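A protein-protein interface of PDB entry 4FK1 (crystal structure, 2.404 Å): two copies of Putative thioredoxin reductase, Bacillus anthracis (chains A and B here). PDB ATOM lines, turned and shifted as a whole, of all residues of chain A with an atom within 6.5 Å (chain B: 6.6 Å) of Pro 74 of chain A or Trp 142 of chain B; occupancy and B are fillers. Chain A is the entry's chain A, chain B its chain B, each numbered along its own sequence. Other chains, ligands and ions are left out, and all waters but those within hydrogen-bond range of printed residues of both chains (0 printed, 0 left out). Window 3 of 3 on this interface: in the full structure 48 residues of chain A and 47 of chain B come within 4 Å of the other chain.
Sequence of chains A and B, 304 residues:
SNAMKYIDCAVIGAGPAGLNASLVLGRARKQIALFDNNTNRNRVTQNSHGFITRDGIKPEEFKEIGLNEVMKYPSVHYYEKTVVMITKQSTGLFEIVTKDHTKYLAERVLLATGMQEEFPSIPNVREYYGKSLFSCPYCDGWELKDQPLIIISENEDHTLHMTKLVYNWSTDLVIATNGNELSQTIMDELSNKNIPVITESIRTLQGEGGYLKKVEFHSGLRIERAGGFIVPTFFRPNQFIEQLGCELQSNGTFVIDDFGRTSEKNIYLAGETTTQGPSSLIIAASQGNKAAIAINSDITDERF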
ATOM      1  N   GLY A  26      20.628  21.927  16.410  1.00  0.00           N
ATOM      2  CA  GLY A  26      21.102  21.243  15.219  1.00  0.00           C
ATOM      3  C   GLY A  26      20.005  20.413  14.571  1.00  0.00           C
ATOM      4  O   GLY A  26      19.879  20.380  13.353  1.00  0.00           O
ATOM      5  N   ARG A  27      19.201  19.746  15.387  1.00  0.00           N
ATOM      6  CA  ARG A  27      18.070  18.996  14.866  1.00  0.00           C
ATOM      7  C   ARG A  27      16.946  19.907  14.332  1.00  0.00           C
ATOM      8  O   ARG A  27      16.101  19.446  13.552  1.00  0.00           O
ATOM      9  CB  ARG A  27      17.518  18.013  15.909  1.00  0.00           C
ATOM     10  CG  ARG A  27      18.404  16.806  16.122  1.00  0.00           C
ATOM     11  CD  ARG A  27      17.940  15.923  17.314  1.00  0.00           C
ATOM     12  NE  ARG A  27      16.566  15.454  17.135  1.00  0.00           N
ATOM     13  CZ  ARG A  27      16.181  14.573  16.210  1.00  0.00           C
ATOM     14  NH1 ARG A  27      17.061  14.033  15.367  1.00  0.00           N
ATOM     15  NH2 ARG A  27      14.909  14.210  16.146  1.00  0.00           N
ATOM     16  N   ALA A  28      16.938  21.172  14.759  1.00  0.00           N
ATOM     17  CA  ALA A  28      15.966  22.164  14.291  1.00  0.00           C
ATOM     18  C   ALA A  28      16.483  22.989  13.090  1.00  0.00           C
ATOM     19  O   ALA A  28      15.923  24.042  12.745  1.00  0.00           O
ATOM     20  CB  ALA A  28      15.564  23.085  15.446  1.00  0.00           C
ATOM     21  N   ARG A  29      17.566  22.508  12.480  1.00  0.00           N
ATOM     22  CA  ARG A  29      18.158  23.098  11.272  1.00  0.00           C
ATOM     23  C   ARG A  29      18.709  24.520  11.427  1.00  0.00           C
ATOM     24  O   ARG A  29      18.719  25.307  10.477  1.00  0.00           O
ATOM     25  CB  ARG A  29      17.171  23.010  10.107  1.00  0.00           C
ATOM     26  CG  ARG A  29      16.486  21.646  10.031  1.00  0.00           C
ATOM     27  CD  ARG A  29      15.447  21.604   8.944  1.00  0.00           C
ATOM     28  NE  ARG A  29      16.062  21.344   7.649  1.00  0.00           N
ATOM     29  CZ  ARG A  29      15.432  21.460   6.489  1.00  0.00           C
ATOM     30  NH1 ARG A  29      14.169  21.857   6.456  1.00  0.00           N
ATOM     31  NH2 ARG A  29      16.076  21.197   5.366  1.00  0.00           N
ATOM     32  N   GLN A  31      21.848  27.257  12.208  1.00  0.00           N
ATOM     33  CA  GLN A  31      23.303  27.356  12.052  1.00  0.00           C
ATOM     34  C   GLN A  31      23.975  27.672  13.390  1.00  0.00           C
ATOM     35  O   GLN A  31      23.767  28.740  13.969  1.00  0.00           O
ATOM     36  CB  GLN A  31      23.669  28.426  11.018  1.00  0.00           C
ATOM     37  CG  GLN A  31      23.328  28.064   9.582  1.00  0.00           C
ATOM     38  CD  GLN A  31      24.050  26.812   9.120  1.00  0.00           C
ATOM     39  OE1 GLN A  31      25.185  26.547   9.525  1.00  0.00           O
ATOM     40  NE2 GLN A  31      23.389  26.027   8.280  1.00  0.00           N
ATOM     41  N   VAL A  70      26.361  15.614  18.410  1.00  0.00           N
ATOM     42  CA  VAL A  70      26.116  16.964  17.939  1.00  0.00           C
ATOM     43  C   VAL A  70      26.638  17.157  16.515  1.00  0.00           C
ATOM     44  O   VAL A  70      25.970  17.753  15.676  1.00  0.00           O
ATOM     45  CB  VAL A  70      26.745  17.972  18.927  1.00  0.00           C
ATOM     46  CG1 VAL A  70      27.523  19.044  18.215  1.00  0.00           C
ATOM     47  CG2 VAL A  70      25.684  18.571  19.815  1.00  0.00           C
ATOM     48  N   MET A  71      27.815  16.612  16.234  1.00  0.00           N
ATOM     49  CA  MET A  71      28.422  16.783  14.922  1.00  0.00           C
ATOM     50  C   MET A  71      27.868  15.850  13.835  1.00  0.00           C
ATOM     51  O   MET A  71      28.391  15.815  12.721  1.00  0.00           O
ATOM     52  CB  MET A  71      29.945  16.679  15.016  1.00  0.00           C
ATOM     53  CG  MET A  71      30.577  17.756  15.890  1.00  0.00           C
ATOM     54  SD  MET A  71      32.397  18.215  15.344  1.00  0.00           S
ATOM     55  CE  MET A  71      31.974  19.435  13.863  1.00  0.00           C
ATOM     56  N   LYS A  72      26.818  15.095  14.143  1.00  0.00           N
ATOM     57  CA  LYS A  72      26.111  14.356  13.098  1.00  0.00           C
ATOM     58  C   LYS A  72      25.329  15.363  12.248  1.00  0.00           C
ATOM     59  O   LYS A  72      25.169  15.197  11.042  1.00  0.00           O
ATOM     60  CB  LYS A  72      25.163  13.315  13.703  1.00  0.00           C
ATOM     61  CG  LYS A  72      25.859  12.190  14.471  1.00  0.00           C
ATOM     62  CD  LYS A  72      24.852  11.170  15.024  1.00  0.00           C
ATOM     63  CE  LYS A  72      23.840  11.825  15.967  1.00  0.00           C
ATOM     64  NZ  LYS A  72      22.793  10.872  16.422  1.00  0.00           N
ATOM     65  N   TYR A  73      24.879  16.425  12.903  1.00  0.00           N
ATOM     66  CA  TYR A  73      24.041  17.447  12.293  1.00  0.00           C
ATOM     67  C   TYR A  73      24.859  18.506  11.566  1.00  0.00           C
ATOM     68  O   TYR A  73      25.647  19.220  12.181  1.00  0.00           O
ATOM     69  CB  TYR A  73      23.109  18.038  13.361  1.00  0.00           C
ATOM     70  CG  TYR A  73      22.298  16.923  13.958  1.00  0.00           C
ATOM     71  CD1 TYR A  73      21.282  16.326  13.223  1.00  0.00           C
ATOM     72  CD2 TYR A  73      22.601  16.397  15.210  1.00  0.00           C
ATOM     73  CE1 TYR A  73      20.552  15.273  13.730  1.00  0.00           C
ATOM     74  CE2 TYR A  73      21.872  15.335  15.726  1.00  0.00           C
ATOM     75  CZ  TYR A  73      20.848  14.778  14.978  1.00  0.00           C
ATOM     76  OH  TYR A  73      20.107  13.726  15.467  1.00  0.00           O
ATOM     77  N   PRO A  74      24.660  18.605  10.240  1.00  0.00           N
ATOM     78  CA  PRO A  74      25.538  19.342   9.323  1.00  0.00           C
ATOM     79  C   PRO A  74      25.620  20.851   9.591  1.00  0.00           C
ATOM     80  O   PRO A  74      26.554  21.500   9.119  1.00  0.00           O
ATOM     81  CB  PRO A  74      24.929  19.050   7.943  1.00  0.00           C
ATOM     82  CG  PRO A  74      23.508  18.701   8.211  1.00  0.00           C
ATOM     83  CD  PRO A  74      23.509  18.005   9.544  1.00  0.00           C
ATOM     84  N   SER A  75      24.672  21.392  10.348  1.00  0.00           N
ATOM     85  CA  SER A  75      24.624  22.824  10.598  1.00  0.00           C
ATOM     86  C   SER A  75      25.355  23.254  11.884  1.00  0.00           C
ATOM     87  O   SER A  75      25.487  24.455  12.153  1.00  0.00           O
ATOM     88  CB  SER A  75      23.170  23.294  10.646  1.00  0.00           C
ATOM     89  OG  SER A  75      22.550  22.870  11.847  1.00  0.00           O
ATOM     90  N   VAL A  76      25.823  22.286  12.676  1.00  0.00           N
ATOM     91  CA  VAL A  76      26.551  22.594  13.909  1.00  0.00           C
ATOM     92  C   VAL A  76      28.055  22.532  13.697  1.00  0.00           C
ATOM     93  O   VAL A  76      28.594  21.481  13.369  1.00  0.00           O
ATOM     94  CB  VAL A  76      26.191  21.628  15.039  1.00  0.00           C
ATOM     95  CG1 VAL A  76      27.015  21.942  16.267  1.00  0.00           C
ATOM     96  CG2 VAL A  76      24.708  21.715  15.356  1.00  0.00           C
ATOM     97  N   HIS A  77      28.738  23.653  13.901  1.00  0.00           N
ATOM     98  CA  HIS A  77      30.182  23.693  13.681  1.00  0.00           C
ATOM     99  C   HIS A  77      30.943  23.905  14.979  1.00  0.00           C
ATOM    100  O   HIS A  77      30.565  24.746  15.801  1.00  0.00           O
ATOM    101  CB  HIS A  77      30.544  24.770  12.663  1.00  0.00           C
ATOM    102  CG  HIS A  77      29.789  24.658  11.377  1.00  0.00           C
ATOM    103  ND1 HIS A  77      30.353  24.157  10.221  1.00  0.00           N
ATOM    104  CD2 HIS A  77      28.513  24.987  11.062  1.00  0.00           C
ATOM    105  CE1 HIS A  77      29.458  24.185   9.251  1.00  0.00           C
ATOM    106  NE2 HIS A  77      28.332  24.682   9.735  1.00  0.00           N
ATOM    107  N   HIS B  49      15.385  10.988  20.390  1.00  0.00           N
ATOM    108  CA  HIS B  49      16.465  11.927  20.093  1.00  0.00           C
ATOM    109  C   HIS B  49      16.443  13.094  21.070  1.00  0.00           C
ATOM    110  O   HIS B  49      15.447  13.312  21.740  1.00  0.00           O
ATOM    111  CB  HIS B  49      16.347  12.463  18.664  1.00  0.00           C
ATOM    112  CG  HIS B  49      16.495  11.418  17.599  1.00  0.00           C
ATOM    113  ND1 HIS B  49      15.422  10.716  17.092  1.00  0.00           N
ATOM    114  CD2 HIS B  49      17.588  10.962  16.941  1.00  0.00           C
ATOM    115  CE1 HIS B  49      15.846   9.871  16.167  1.00  0.00           C
ATOM    116  NE2 HIS B  49      17.156   9.995  16.060  1.00  0.00           N
ATOM    117  N   PRO B 137       7.535  18.330  17.131  1.00  0.00           N
ATOM    118  CA  PRO B 137       8.495  18.700  16.090  1.00  0.00           C
ATOM    119  C   PRO B 137       9.940  18.730  16.590  1.00  0.00           C
ATOM    120  O   PRO B 137      10.845  18.396  15.838  1.00  0.00           O
ATOM    121  CB  PRO B 137       8.036  20.105  15.707  1.00  0.00           C
ATOM    122  CG  PRO B 137       6.555  20.065  15.951  1.00  0.00           C
ATOM    123  CD  PRO B 137       6.384  19.252  17.177  1.00  0.00           C
ATOM    124  N   TYR B 138      10.159  19.141  17.828  1.00  0.00           N
ATOM    125  CA  TYR B 138      11.505  19.106  18.385  1.00  0.00           C
ATOM    126  C   TYR B 138      12.036  17.664  18.483  1.00  0.00           C
ATOM    127  O   TYR B 138      13.220  17.411  18.292  1.00  0.00           O
ATOM    128  CB  TYR B 138      11.549  19.815  19.746  1.00  0.00           C
ATOM    129  CG  TYR B 138      11.379  21.318  19.634  1.00  0.00           C
ATOM    130  CD1 TYR B 138      12.337  22.093  18.986  1.00  0.00           C
ATOM    131  CD2 TYR B 138      10.264  21.961  20.171  1.00  0.00           C
ATOM    132  CE1 TYR B 138      12.197  23.450  18.878  1.00  0.00           C
ATOM    133  CE2 TYR B 138      10.116  23.328  20.064  1.00  0.00           C
ATOM    134  CZ  TYR B 138      11.090  24.064  19.413  1.00  0.00           C
ATOM    135  OH  TYR B 138      10.970  25.424  19.289  1.00  0.00           O
ATOM    136  N   CYS B 139      11.153  16.712  18.755  1.00  0.00           N
ATOM    137  CA  CYS B 139      11.605  15.336  18.913  1.00  0.00           C
ATOM    138  C   CYS B 139      11.796  14.686  17.550  1.00  0.00           C
ATOM    139  O   CYS B 139      12.814  14.039  17.312  1.00  0.00           O
ATOM    140  CB  CYS B 139      10.647  14.520  19.798  1.00  0.00           C
ATOM    141  SG  CYS B 139      10.452  15.159  21.485  1.00  0.00           S
ATOM    142  N   ASP B 140      10.840  14.899  16.644  1.00  0.00           N
ATOM    143  CA  ASP B 140      10.779  14.106  15.416  1.00  0.00           C
ATOM    144  C   ASP B 140      10.798  14.882  14.115  1.00  0.00           C
ATOM    145  O   ASP B 140      10.620  14.295  13.041  1.00  0.00           O
ATOM    146  CB  ASP B 140       9.557  13.179  15.442  1.00  0.00           C
ATOM    147  CG  ASP B 140       9.633  12.165  16.562  1.00  0.00           C
ATOM    148  OD1 ASP B 140       9.038  12.425  17.635  1.00  0.00           O
ATOM    149  OD2 ASP B 140      10.310  11.123  16.376  1.00  0.00           O
ATOM    150  N   GLY B 141      11.024  16.190  14.198  1.00  0.00           N
ATOM    151  CA  GLY B 141      11.076  17.026  13.004  1.00  0.00           C
ATOM    152  C   GLY B 141      12.200  16.667  12.048  1.00  0.00           C
ATOM    153  O   GLY B 141      11.993  16.617  10.830  1.00  0.00           O
ATOM    154  N   TRP B 142      13.388  16.425  12.594  1.00  0.00           N
ATOM    155  CA  TRP B 142      14.576  16.154  11.789  1.00  0.00           C
ATOM    156  C   TRP B 142      14.369  15.031  10.780  1.00  0.00           C
ATOM    157  O   TRP B 142      14.671  15.169   9.583  1.00  0.00           O
ATOM    158  CB  TRP B 142      15.759  15.793  12.683  1.00  0.00           C
ATOM    159  CG  TRP B 142      16.979  15.528  11.892  1.00  0.00           C
ATOM    160  CD1 TRP B 142      17.539  14.312  11.624  1.00  0.00           C
ATOM    161  CD2 TRP B 142      17.791  16.504  11.219  1.00  0.00           C
ATOM    162  NE1 TRP B 142      18.666  14.470  10.843  1.00  0.00           N
ATOM    163  CE2 TRP B 142      18.839  15.802  10.577  1.00  0.00           C
ATOM    164  CE3 TRP B 142      17.746  17.900  11.115  1.00  0.00           C
ATOM    165  CZ2 TRP B 142      19.829  16.455   9.833  1.00  0.00           C
ATOM    166  CZ3 TRP B 142      18.729  18.548  10.365  1.00  0.00           C
ATOM    167  CH2 TRP B 142      19.759  17.821   9.737  1.00  0.00           C
ATOM    168  N   GLU B 143      13.860  13.912  11.291  1.00  0.00           N
ATOM    169  CA  GLU B 143      13.607  12.732  10.485  1.00  0.00           C
ATOM    170  C   GLU B 143      12.521  12.947   9.422  1.00  0.00           C
ATOM    171  O   GLU B 143      12.376  12.137   8.504  1.00  0.00           O
ATOM    172  CB  GLU B 143      13.253  11.565  11.393  1.00  0.00           C
ATOM    173  CG  GLU B 143      14.473  10.911  12.067  1.00  0.00           C
ATOM    174  CD  GLU B 143      15.080  11.727  13.220  1.00  0.00           C
ATOM    175  OE1 GLU B 143      14.328  12.357  13.994  1.00  0.00           O
ATOM    176  OE2 GLU B 143      16.321  11.725  13.361  1.00  0.00           O
ATOM    177  N   LEU B 144      11.770  14.040   9.539  1.00  0.00           N
ATOM    178  CA  LEU B 144      10.660  14.319   8.619  1.00  0.00           C
ATOM    179  C   LEU B 144      10.924  15.540   7.738  1.00  0.00           C
ATOM    180  O   LEU B 144      10.017  16.028   7.079  1.00  0.00           O
ATOM    181  CB  LEU B 144       9.369  14.554   9.410  1.00  0.00           C
ATOM    182  CG  LEU B 144       8.190  13.573   9.371  1.00  0.00           C
ATOM    183  CD1 LEU B 144       8.623  12.126   9.361  1.00  0.00           C
ATOM    184  CD2 LEU B 144       7.259  13.846  10.555  1.00  0.00           C
ATOM    185  N   LYS B 145      12.151  16.049   7.742  1.00  0.00           N
ATOM    186  CA  LYS B 145      12.402  17.338   7.112  1.00  0.00           C
ATOM    187  C   LYS B 145      12.164  17.302   5.602  1.00  0.00           C
ATOM    188  O   LYS B 145      12.427  16.288   4.948  1.00  0.00           O
ATOM    189  CB  LYS B 145      13.793  17.864   7.461  1.00  0.00           C
ATOM    190  CG  LYS B 145      14.949  17.045   6.949  1.00  0.00           C
ATOM    191  CD  LYS B 145      16.215  17.406   7.711  1.00  0.00           C
ATOM    192  CE  LYS B 145      17.455  16.865   7.040  1.00  0.00           C
ATOM    193  NZ  LYS B 145      17.909  17.827   6.001  1.00  0.00           N
ATOM    194  N   ASP B 146      11.611  18.398   5.082  1.00  0.00           N
ATOM    195  CA  ASP B 146      11.379  18.572   3.655  1.00  0.00           C
ATOM    196  C   ASP B 146      10.416  17.550   3.054  1.00  0.00           C
ATOM    197  O   ASP B 146      10.527  17.185   1.889  1.00  0.00           O
ATOM    198  CB  ASP B 146      12.710  18.569   2.901  1.00  0.00           C
ATOM    199  CG  ASP B 146      13.613  19.705   3.325  1.00  0.00           C
ATOM    200  OD1 ASP B 146      13.080  20.756   3.742  1.00  0.00           O
ATOM    201  OD2 ASP B 146      14.854  19.552   3.240  1.00  0.00           O
ATOM    202  N   TRP B 169      10.673  22.615   9.704  1.00  0.00           N
ATOM    203  CA  TRP B 169      11.171  21.349   9.163  1.00  0.00           C
ATOM    204  C   TRP B 169      10.684  21.066   7.754  1.00  0.00           C
ATOM    205  O   TRP B 169      11.428  20.535   6.934  1.00  0.00           O
ATOM    206  CB  TRP B 169      10.857  20.181  10.100  1.00  0.00           C
ATOM    207  CG  TRP B 169      11.710  20.195  11.339  1.00  0.00           C
ATOM    208  CD1 TRP B 169      12.929  19.593  11.502  1.00  0.00           C
ATOM    209  CD2 TRP B 169      11.423  20.855  12.579  1.00  0.00           C
ATOM    210  NE1 TRP B 169      13.403  19.822  12.757  1.00  0.00           N
ATOM    211  CE2 TRP B 169      12.504  20.589  13.445  1.00  0.00           C
ATOM    212  CE3 TRP B 169      10.358  21.631  13.042  1.00  0.00           C
ATOM    213  CZ2 TRP B 169      12.558  21.090  14.750  1.00  0.00           C
ATOM    214  CZ3 TRP B 169      10.411  22.120  14.341  1.00  0.00           C
ATOM    215  CH2 TRP B 169      11.506  21.847  15.178  1.00  0.00           C
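Lys 72 of chain A touches none of the printed residues of chain B.
Of the printed residues of chain B, Pro 74 of chain A touches Trp 142.
Printed residues of chain A within 4 Å of Trp 142 of chain B: Gly 26, Arg 27, Arg 29, Tyr 73 and Pro 74.
Printed residues of chain A within 4 Å of Glu 143 of chain B: Arg 27 (2.9 Å).
Of the printed residues of chain A, Trp 169 of chain B touches Arg 27 (2.8 Å), Ala 28 (3.6 Å) and Arg 29 (3.1 Å).
The nearest residue of chain B that does not touch Pro 74 of chain A is Lys 145 of chain B (6.1 Å).
The nearest printed residue of chain A that does not touch Asp 146 of chain B is Arg 27 of chain A (9.6 Å).
Of the 13 printed residues of chain A, 6 touch a printed residue of chain B.
Of the 12 printed residues of chain B, 7 touch a printed residue of chain A.
Printed residues of chain B that touch a printed residue of chain A: His 49, Cys 139, Trp 142, Glu 143, Lys 145, Asp 146 and Trp 169.
Hydrophobic or aromatic side chains of chain B that line the printed part of chain A: His 49, Trp 142 and Trp 169.
Among the printed residues, 13 pairs touch across the chains.
OH of Tyr 73 of chain A is in hydrogen-bond range of NH1 of Arg 27 of chain A.
A ring nitrogen (NE2) of His 49 of chain B lies within hydrogen-bond range of the side-chain carboxylate (OE2) of Glu 143 of chain B (3.3 Å).
The backbone NH (N) of Asp 146 of chain B is in hydrogen-bond range of the backbone carbonyl oxygen (O) of Trp 169 of chain B.
No position is printed for both chains.
Of the 13 pairs that touch across the chains among the printed residues, none has its exchanged pair printed and touching as well.
NH2 of Arg 27 of chain A lies within hydrogen-bond range of O of Cys 139 of chain B, 2.4 Å away.
The side-chain carboxylate (OE1) of Glu 143 of chain B is in salt-bridge range of the guanidinium group (NH2) of Arg 27 of chain A, at 2.9 Å.
O of Arg 27 of chain A is in hydrogen-bond range of NE1 of Trp 169 of chain B (2.8 Å).
NH2 of Arg 29 of chain A lies within salt-bridge range of OD2 of Asp 146 of chain B (3.0 Å).
The backbone carbonyl oxygen of Trp 169 of chain B lies within hydrogen-bond range of the guanidinium group of Arg 29 of chain A (3.1 Å).
CZ3 of Trp 142 of chain B touches O of Gly 26 of chain A (3.7 Å).
His 49 of chain B touches Arg 27 of chain A (CB to CZ, 3.2 Å).
O of Arg 27 of chain A touches CE3 of Trp 142 of chain B, at 3.3 Å.
Ala 28 of chain A touches Trp 169 of chain B.
Trp 142 of chain B touches Arg 29 of chain A.
Lys 145 of chain B touches Arg 29 of chain A.
CE1 of Tyr 73 of chain A touches NE1 of Trp 142 of chain B, at 3.5 Å.
Pro 74 of chain A touches Trp 142 of chain B (CD to CH2, 3.8 Å).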
